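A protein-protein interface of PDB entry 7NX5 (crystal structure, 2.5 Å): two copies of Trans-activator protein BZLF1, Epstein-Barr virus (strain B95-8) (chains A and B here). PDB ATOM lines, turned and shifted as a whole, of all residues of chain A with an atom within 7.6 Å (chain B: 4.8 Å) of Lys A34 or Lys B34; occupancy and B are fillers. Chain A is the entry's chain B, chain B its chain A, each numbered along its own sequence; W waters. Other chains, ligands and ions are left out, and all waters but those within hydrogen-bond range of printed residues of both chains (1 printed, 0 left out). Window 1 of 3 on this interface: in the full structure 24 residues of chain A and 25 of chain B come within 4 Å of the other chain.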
ATOM      1  N   GLU A  29      12.295   0.166  26.248  1.00  0.00           N
ATOM      2  CA  GLU A  29      12.613   1.121  25.195  1.00  0.00           C
ATOM      3  C   GLU A  29      11.739   2.358  25.312  1.00  0.00           C
ATOM      4  O   GLU A  29      12.249   3.467  25.508  1.00  0.00           O
ATOM      5  CB  GLU A  29      12.470   0.430  23.846  1.00  0.00           C
ATOM      6  CG  GLU A  29      13.653  -0.473  23.602  1.00  0.00           C
ATOM      7  CD  GLU A  29      13.387  -1.495  22.543  1.00  0.00           C
ATOM      8  OE1 GLU A  29      12.768  -1.108  21.538  1.00  0.00           O
ATOM      9  OE2 GLU A  29      13.775  -2.677  22.718  1.00  0.00           O
ATOM     10  N   VAL A  30      10.417   2.160  25.279  1.00  0.00           N
ATOM     11  CA  VAL A  30       9.447   3.216  25.557  1.00  0.00           C
ATOM     12  C   VAL A  30       9.843   4.068  26.766  1.00  0.00           C
ATOM     13  O   VAL A  30       9.688   5.301  26.755  1.00  0.00           O
ATOM     14  CB  VAL A  30       8.049   2.607  25.735  1.00  0.00           C
ATOM     15  CG1 VAL A  30       7.130   3.567  26.502  1.00  0.00           C
ATOM     16  CG2 VAL A  30       7.479   2.267  24.374  1.00  0.00           C
ATOM     17  N   ALA A  31      10.399   3.443  27.803  1.00  0.00           N
ATOM     18  CA  ALA A  31      10.806   4.232  28.955  1.00  0.00           C
ATOM     19  C   ALA A  31      11.912   5.211  28.580  1.00  0.00           C
ATOM     20  O   ALA A  31      11.861   6.399  28.930  1.00  0.00           O
ATOM     21  CB  ALA A  31      11.234   3.309  30.099  1.00  0.00           C
ATOM     22  N   ALA A  32      12.911   4.742  27.837  1.00  0.00           N
ATOM     23  CA  ALA A  32      14.015   5.627  27.471  1.00  0.00           C
ATOM     24  C   ALA A  32      13.563   6.706  26.495  1.00  0.00           C
ATOM     25  O   ALA A  32      13.953   7.870  26.626  1.00  0.00           O
ATOM     26  CB  ALA A  32      15.167   4.813  26.879  1.00  0.00           C
ATOM     27  N   ALA A  33      12.766   6.322  25.496  1.00  0.00           N
ATOM     28  CA  ALA A  33      12.266   7.275  24.507  1.00  0.00           C
ATOM     29  C   ALA A  33      11.495   8.411  25.168  1.00  0.00           C
ATOM     30  O   ALA A  33      11.766   9.594  24.925  1.00  0.00           O
ATOM     31  CB  ALA A  33      11.384   6.551  23.496  1.00  0.00           C
ATOM     32  N   LYS A  34      10.536   8.075  26.041  1.00  0.00           N
ATOM     33  CA  LYS A  34       9.782   9.135  26.704  1.00  0.00           C
ATOM     34  C   LYS A  34      10.645   9.937  27.659  1.00  0.00           C
ATOM     35  O   LYS A  34      10.441  11.148  27.789  1.00  0.00           O
ATOM     36  CB  LYS A  34       8.547   8.552  27.389  1.00  0.00           C
ATOM     37  CG  LYS A  34       7.649   7.855  26.365  1.00  0.00           C
ATOM     38  CD  LYS A  34       6.171   8.170  26.528  1.00  0.00           C
ATOM     39  CE  LYS A  34       5.339   7.435  25.480  1.00  0.00           C
ATOM     40  NZ  LYS A  34       4.421   8.378  24.760  1.00  0.00           N
ATOM     41  N   SER A  35      11.656   9.326  28.284  1.00  0.00           N
ATOM     42  CA  SER A  35      12.481  10.098  29.217  1.00  0.00           C
ATOM     43  C   SER A  35      13.385  11.090  28.485  1.00  0.00           C
ATOM     44  O   SER A  35      13.547  12.236  28.923  1.00  0.00           O
ATOM     45  CB  SER A  35      13.292   9.149  30.097  1.00  0.00           C
ATOM     46  OG  SER A  35      12.482   8.041  30.475  1.00  0.00           O
ATOM     47  N   SER A  36      13.979  10.683  27.369  1.00  0.00           N
ATOM     48  CA  SER A  36      14.745  11.644  26.574  1.00  0.00           C
ATOM     49  C   SER A  36      13.851  12.773  26.054  1.00  0.00           C
ATOM     50  O   SER A  36      14.225  13.952  26.118  1.00  0.00           O
ATOM     51  CB  SER A  36      15.430  10.940  25.414  1.00  0.00           C
ATOM     52  OG  SER A  36      14.445  10.399  24.561  1.00  0.00           O
ATOM     53  N   GLU A  37      12.677  12.426  25.502  1.00  0.00           N
ATOM     54  CA  GLU A  37      11.725  13.450  25.077  1.00  0.00           C
ATOM     55  C   GLU A  37      11.420  14.430  26.206  1.00  0.00           C
ATOM     56  O   GLU A  37      11.345  15.647  25.982  1.00  0.00           O
ATOM     57  CB  GLU A  37      10.439  12.795  24.577  1.00  0.00           C
ATOM     58  CG  GLU A  37       9.358  13.794  24.229  1.00  0.00           C
ATOM     59  CD  GLU A  37       8.055  13.155  23.794  1.00  0.00           C
ATOM     60  OE1 GLU A  37       8.091  11.975  23.378  1.00  0.00           O
ATOM     61  OE2 GLU A  37       6.996  13.832  23.875  1.00  0.00           O
ATOM     62  N   ASN A  38      11.256  13.910  27.434  1.00  0.00           N
ATOM     63  CA  ASN A  38      11.006  14.738  28.617  1.00  0.00           C
ATOM     64  C   ASN A  38      12.164  15.699  28.871  1.00  0.00           C
ATOM     65  O   ASN A  38      11.963  16.872  29.207  1.00  0.00           O
ATOM     66  CB  ASN A  38      10.788  13.788  29.824  1.00  0.00           C
ATOM     67  CG  ASN A  38      10.274  14.493  31.085  1.00  0.00           C
ATOM     68  OD1 ASN A  38      11.008  15.184  31.799  1.00  0.00           O
ATOM     69  ND2 ASN A  38       9.008  14.290  31.366  1.00  0.00           N
ATOM     70  N   ASP A  39      13.389  15.200  28.730  1.00  0.00           N
ATOM     71  CA  ASP A  39      14.581  16.030  28.893  1.00  0.00           C
ATOM     72  C   ASP A  39      14.664  17.119  27.835  1.00  0.00           C
ATOM     73  O   ASP A  39      15.015  18.268  28.141  1.00  0.00           O
ATOM     74  CB  ASP A  39      15.823  15.157  28.834  1.00  0.00           C
ATOM     75  CG  ASP A  39      15.744  13.996  29.789  1.00  0.00           C
ATOM     76  OD1 ASP A  39      15.096  14.145  30.851  1.00  0.00           O
ATOM     77  OD2 ASP A  39      16.315  12.931  29.474  1.00  0.00           O
ATOM     78  N   ARG A  40      14.337  16.792  26.585  1.00  0.00           N
ATOM     79  CA  ARG A  40      14.472  17.824  25.554  1.00  0.00           C
ATOM     80  C   ARG A  40      13.354  18.843  25.648  1.00  0.00           C
ATOM     81  O   ARG A  40      13.540  20.002  25.286  1.00  0.00           O
ATOM     82  CB  ARG A  40      14.509  17.202  24.173  1.00  0.00           C
ATOM     83  CG  ARG A  40      15.353  15.965  24.143  1.00  0.00           C
ATOM     84  CD  ARG A  40      14.709  14.972  23.243  1.00  0.00           C
ATOM     85  NE  ARG A  40      14.530  15.561  21.929  1.00  0.00           N
ATOM     86  CZ  ARG A  40      15.426  15.467  20.955  1.00  0.00           C
ATOM     87  NH1 ARG A  40      16.550  14.788  21.158  1.00  0.00           N
ATOM     88  NH2 ARG A  40      15.199  16.044  19.779  1.00  0.00           N
ATOM     89  N   LEU A  41      12.194  18.437  26.148  1.00  0.00           N
ATOM     90  CA  LEU A  41      11.121  19.398  26.331  1.00  0.00           C
ATOM     91  C   LEU A  41      11.446  20.337  27.470  1.00  0.00           C
ATOM     92  O   LEU A  41      11.281  21.556  27.340  1.00  0.00           O
ATOM     93  CB  LEU A  41       9.794  18.688  26.592  1.00  0.00           C
ATOM     94  CG  LEU A  41       9.140  17.810  25.520  1.00  0.00           C
ATOM     95  CD1 LEU A  41       8.299  16.781  26.226  1.00  0.00           C
ATOM     96  CD2 LEU A  41       8.287  18.598  24.587  1.00  0.00           C
ATOM     97  N   ARG A  42      11.911  19.801  28.599  1.00  0.00           N
ATOM     98  CA  ARG A  42      12.343  20.711  29.649  1.00  0.00           C
ATOM     99  C   ARG A  42      13.440  21.642  29.131  1.00  0.00           C
ATOM    100  O   ARG A  42      13.360  22.856  29.324  1.00  0.00           O
ATOM    101  CB  ARG A  42      12.791  19.934  30.884  1.00  0.00           C
ATOM    102  CG  ARG A  42      11.639  19.467  31.732  1.00  0.00           C
ATOM    103  CD  ARG A  42      12.064  18.632  32.960  1.00  0.00           C
ATOM    104  NE  ARG A  42      10.972  17.817  33.522  1.00  0.00           N
ATOM    105  CZ  ARG A  42      10.007  18.312  34.277  1.00  0.00           C
ATOM    106  NH1 ARG A  42      10.002  19.606  34.571  1.00  0.00           N
ATOM    107  NH2 ARG A  42       9.054  17.528  34.744  1.00  0.00           N
ATOM    108  N   ARG A  60       9.602  16.984  38.074  1.00  0.00           N
ATOM    109  CA  ARG A  60      10.180  15.782  37.501  1.00  0.00           C
ATOM    110  C   ARG A  60       9.812  14.591  38.366  1.00  0.00           C
ATOM    111  O   ARG A  60       9.725  14.695  39.590  1.00  0.00           O
ATOM    112  CB  ARG A  60      11.701  15.885  37.407  1.00  0.00           C
ATOM    113  CG  ARG A  60      12.231  16.856  36.384  1.00  0.00           C
ATOM    114  CD  ARG A  60      13.733  16.819  36.393  1.00  0.00           C
ATOM    115  NE  ARG A  60      14.317  17.972  35.725  1.00  0.00           N
ATOM    116  CZ  ARG A  60      15.625  18.156  35.573  1.00  0.00           C
ATOM    117  NH1 ARG A  60      16.479  17.253  36.040  1.00  0.00           N
ATOM    118  NH2 ARG A  60      16.081  19.231  34.936  1.00  0.00           N
ATOM    119  N   THR A  61       9.577  13.466  37.723  1.00  0.00           N
ATOM    120  CA  THR A  61       9.447  12.213  38.427  1.00  0.00           C
ATOM    121  C   THR A  61      10.780  11.501  38.337  1.00  0.00           C
ATOM    122  O   THR A  61      11.228  11.217  37.212  1.00  0.00           O
ATOM    123  CB  THR A  61       8.348  11.365  37.805  1.00  0.00           C
ATOM    124  OG1 THR A  61       7.069  11.898  38.175  1.00  0.00           O
ATOM    125  CG2 THR A  61       8.465   9.895  38.208  1.00  0.00           C
ATOM    126  N   PRO A  62      11.458  11.230  39.456  1.00  0.00           N
ATOM    127  CA  PRO A  62      12.789  10.608  39.385  1.00  0.00           C
ATOM    128  C   PRO A  62      12.823   9.429  38.415  1.00  0.00           C
ATOM    129  O   PRO A  62      11.865   8.657  38.310  1.00  0.00           O
ATOM    130  CB  PRO A  62      13.054  10.177  40.831  1.00  0.00           C
ATOM    131  CG  PRO A  62      12.268  11.157  41.656  1.00  0.00           C
ATOM    132  CD  PRO A  62      11.048  11.518  40.846  1.00  0.00           C
ATOM    133  N   ASP A  63      13.934   9.361  37.676  1.00  0.00           N
ATOM    134  CA  ASP A  63      14.299   8.468  36.555  1.00  0.00           C
ATOM    135  C   ASP A  63      14.274   9.292  35.274  1.00  0.00           C
ATOM    136  O   ASP A  63      13.266   9.914  34.947  1.00  0.00           O
ATOM    137  CB  ASP A  63      13.417   7.223  36.384  1.00  0.00           C
ATOM    138  CG  ASP A  63      14.091   6.163  35.505  1.00  0.00           C
ATOM    139  OD1 ASP A  63      15.236   6.410  35.080  1.00  0.00           O
ATOM    140  OD2 ASP A  63      13.505   5.092  35.236  1.00  0.00           O
ATOM    141  OXT ASP A  63      15.278   9.374  34.558  1.00  0.00           O
ATOM    142  N   VAL B  30       7.388   4.052  34.740  1.00  0.00           N
ATOM    143  CA  VAL B  30       8.225   5.141  34.235  1.00  0.00           C
ATOM    144  C   VAL B  30       7.642   5.712  32.943  1.00  0.00           C
ATOM    145  O   VAL B  30       7.548   6.930  32.760  1.00  0.00           O
ATOM    146  CB  VAL B  30       9.665   4.650  34.013  1.00  0.00           C
ATOM    147  CG1 VAL B  30      10.414   5.606  33.069  1.00  0.00           C
ATOM    148  CG2 VAL B  30      10.390   4.511  35.357  1.00  0.00           C
ATOM    149  N   ALA B  31       7.277   4.829  32.019  1.00  0.00           N
ATOM    150  CA  ALA B  31       6.547   5.219  30.825  1.00  0.00           C
ATOM    151  C   ALA B  31       5.321   6.051  31.172  1.00  0.00           C
ATOM    152  O   ALA B  31       5.065   7.084  30.550  1.00  0.00           O
ATOM    153  CB  ALA B  31       6.133   3.974  30.061  1.00  0.00           C
ATOM    154  N   ALA B  32       4.538   5.596  32.152  1.00  0.00           N
ATOM    155  CA  ALA B  32       3.324   6.317  32.522  1.00  0.00           C
ATOM    156  C   ALA B  32       3.653   7.729  32.965  1.00  0.00           C
ATOM    157  O   ALA B  32       3.137   8.718  32.418  1.00  0.00           O
ATOM    158  CB  ALA B  32       2.599   5.567  33.640  1.00  0.00           C
ATOM    159  N   ALA B  33       4.509   7.827  33.982  1.00  0.00           N
ATOM    160  CA  ALA B  33       4.885   9.119  34.533  1.00  0.00           C
ATOM    161  C   ALA B  33       5.381  10.028  33.430  1.00  0.00           C
ATOM    162  O   ALA B  33       5.004  11.205  33.353  1.00  0.00           O
ATOM    163  CB  ALA B  33       5.962   8.937  35.614  1.00  0.00           C
ATOM    164  N   LYS B  34       6.199   9.469  32.544  1.00  0.00           N
ATOM    165  CA  LYS B  34       6.858  10.250  31.525  1.00  0.00           C
ATOM    166  C   LYS B  34       5.841  10.787  30.528  1.00  0.00           C
ATOM    167  O   LYS B  34       5.764  11.998  30.323  1.00  0.00           O
ATOM    168  CB  LYS B  34       7.939   9.417  30.836  1.00  0.00           C
ATOM    169  CG  LYS B  34       9.213   9.256  31.669  1.00  0.00           C
ATOM    170  CD  LYS B  34       9.972  10.556  31.835  1.00  0.00           C
ATOM    171  CE  LYS B  34      11.231  10.361  32.658  1.00  0.00           C
ATOM    172  NZ  LYS B  34      10.928  10.217  34.122  1.00  0.00           N
ATOM    173  N   SER B  35       5.036   9.902  29.933  1.00  0.00           N
ATOM    174  CA  SER B  35       4.047  10.355  28.958  1.00  0.00           C
ATOM    175  C   SER B  35       3.148  11.446  29.532  1.00  0.00           C
ATOM    176  O   SER B  35       2.797  12.405  28.825  1.00  0.00           O
ATOM    177  CB  SER B  35       3.216   9.181  28.470  1.00  0.00           C
ATOM    178  OG  SER B  35       2.174   9.655  27.636  1.00  0.00           O
ATOM    179  N   SER B  36       2.799  11.356  30.819  1.00  0.00           N
ATOM    180  CA  SER B  36       1.965  12.398  31.407  1.00  0.00           C
ATOM    181  C   SER B  36       2.714  13.736  31.520  1.00  0.00           C
ATOM    182  O   SER B  36       2.221  14.795  31.072  1.00  0.00           O
ATOM    183  CB  SER B  36       1.456  11.938  32.767  1.00  0.00           C
ATOM    184  OG  SER B  36       0.753  12.973  33.421  1.00  0.00           O
ATOM    185  N   GLU B  37       3.899  13.711  32.140  1.00  0.00           N
ATOM    186  CA  GLU B  37       4.747  14.899  32.129  1.00  0.00           C
ATOM    187  C   GLU B  37       4.906  15.443  30.714  1.00  0.00           C
ATOM    188  O   GLU B  37       4.960  16.657  30.507  1.00  0.00           O
ATOM    189  CB  GLU B  37       6.134  14.589  32.685  1.00  0.00           C
ATOM    190  CG  GLU B  37       6.249  14.202  34.130  1.00  0.00           C
ATOM    191  CD  GLU B  37       7.607  13.585  34.450  1.00  0.00           C
ATOM    192  OE1 GLU B  37       8.647  14.064  33.941  1.00  0.00           O
ATOM    193  OE2 GLU B  37       7.624  12.594  35.212  1.00  0.00           O
ATOM    194  N   ASN B  38       5.011  14.548  29.737  1.00  0.00           N
ATOM    195  CA  ASN B  38       5.324  14.946  28.370  1.00  0.00           C
ATOM    196  C   ASN B  38       4.203  15.787  27.793  1.00  0.00           C
ATOM    197  O   ASN B  38       4.446  16.850  27.222  1.00  0.00           O
ATOM    198  CB  ASN B  38       5.561  13.713  27.487  1.00  0.00           C
ATOM    199  CG  ASN B  38       6.958  13.153  27.601  1.00  0.00           C
ATOM    200  OD1 ASN B  38       7.838  13.743  28.226  1.00  0.00           O
ATOM    201  ND2 ASN B  38       7.174  12.002  26.963  1.00  0.00           N
ATOM    202  N   THR B  61       6.952  10.382  20.950  1.00  0.00           N
ATOM    203  CA  THR B  61       7.405   9.004  20.989  1.00  0.00           C
ATOM    204  C   THR B  61       6.221   8.067  21.203  1.00  0.00           C
ATOM    205  O   THR B  61       5.246   8.427  21.871  1.00  0.00           O
ATOM    206  CB  THR B  61       8.417   8.811  22.111  1.00  0.00           C
ATOM    207  OG1 THR B  61       7.875   9.319  23.341  1.00  0.00           O
ATOM    208  CG2 THR B  61       9.707   9.532  21.779  1.00  0.00           C
ATOM    209  N   PRO B  62       6.270   6.851  20.652  1.00  0.00           N
ATOM    210  CA  PRO B  62       5.091   5.985  20.732  1.00  0.00           C
ATOM    211  C   PRO B  62       4.848   5.430  22.153  1.00  0.00           C
ATOM    212  O   PRO B  62       3.756   4.971  22.497  1.00  0.00           O
ATOM    213  CB  PRO B  62       5.426   4.878  19.739  1.00  0.00           C
ATOM    214  CG  PRO B  62       6.921   4.827  19.728  1.00  0.00           C
ATOM    215  CD  PRO B  62       7.408   6.207  19.975  1.00  0.00           C
HETATM  216  O   HOH W   1       2.943  11.383  25.620  1.00  0.00           O
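Water W1 lies within hydrogen-bond range of the side-chain hydroxyl (OG) of Ser B35 and the side-chain amino group (NZ) of Lys A34.
The side-chain amide nitrogen (ND2) of Asn B38 sits at hydrogen-bond distance from the backbone carbonyl oxygen (O) of Lys A34 (3.5 Å). NZ of Lys B34 is in salt-bridge range of O of Asp A63, 2.5 Å away. The side-chain carboxylate (OE2) of Glu B37 lies close to the side-chain hydroxyl (OG1) of Thr A61 (3.1 Å). NZ of Lys B34 sits at hydrogen-bond distance from O of Thr A61, 3.3 Å away. The side-chain carboxylate (OE1) of Glu A37 lies within hydrogen-bond range of the side-chain hydroxyl (OG1) of Thr B61. OE1 of Glu B37 is in salt-bridge range of NH2 of Arg A42 (3.6 Å). The side-chain carboxylate (OE1) of Glu B37 is in hydrogen-bond range of the side-chain amide nitrogen (ND2) of Asn A38 (2.6 Å). O of Thr B61 lies within hydrogen-bond range of NZ of Lys A34. The side-chain amide nitrogen (ND2) of Asn A38 lies close to the side-chain amide oxygen (OD1) of Asn B38 (3.4 Å).
Lys B34 touches just these residues of chain A: Lys A34, Ser A35, Asn A38, Thr A61 and Asp A63. Ala B33 touches just one residue of chain A: Thr A61. Of the printed residues of chain B, Val A30 touches Ala B31. Printed residues of chain B within 4 Å of Arg A42: Glu B37 (3.6 Å). Printed residues of chain B within 4 Å of Asp A63: Val B30 and Lys B34. Printed residues of chain B within 4 Å of Asn A38: Lys B34, Glu B37 and Asn B38. Asp A39 touches none of the printed residues of chain B. Ala B32 touches none of the printed residues of chain A. The nearest residue of chain B that does not touch Lys A34 is Ala B31 (4.3 Å). The nearest printed residue of chain B that does not touch Thr A61 is Val B30 (6.2 Å).
Among the printed residues, pairs that only touch across the chains: Val A30 with Ala B31, Ala A31 with Val B30, Ala A33 with Thr B61, Lys A34 with Lys B34, Lys A34 with Ser B35, Lys A34 with Pro B62, Ser A35 with Lys B34, Glu A37 with Asn B38, Asn A38 with Lys B34, Leu A41 with Asn B38, Thr A61 with Ala B33 and Asp A63 with Val B30.
Printed residues of chain A that touch a printed residue of chain B: Val A30, Ala A31, Ala A33, Lys A34, Ser A35, Glu A37, Asn A38, Leu A41, Arg A42, Thr A61 and Asp A63. Hydrophobic or aromatic side chains of chain A within 4 Å of the printed part of chain B: Val A30, Ala A31, Ala A33 and Leu A41. Of the 11 printed residues of chain B, 9 touch a printed residue of chain A. Among the printed residues, 21 pairs touch across the chains.
Val A30 touches Ala B31, and with the chains exchanged Ala A31 touches Val B30. Lys B34 touches its own counterpart, Lys A34. Lys A34 touches Pro B62, but with the chains exchanged Pro A62 does not touch Lys B34 (4.6 Å). Glu A37 touches Asn B38, and with the chains exchanged Asn A38 touches Glu B37. Positions printed for both chains: 30, 31, 32, 33, 34, 35, 36, 37, 38, 61 and 62. Of the 21 pairs that touch across the chains among the printed residues, 16 have their exchanged pair printed and touching as well.
The backbone carbonyl oxygen (O) of Ala A33 sits at hydrogen-bond distance from the side-chain hydroxyl (OG) of Ser A36, 2.8 Å away. O of Lys B34 lies close to OD1 of Asn B38 (3.4 Å). OD1 of Asn A38 sits at hydrogen-bond distance from NE of Arg A42, 3.1 Å away.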
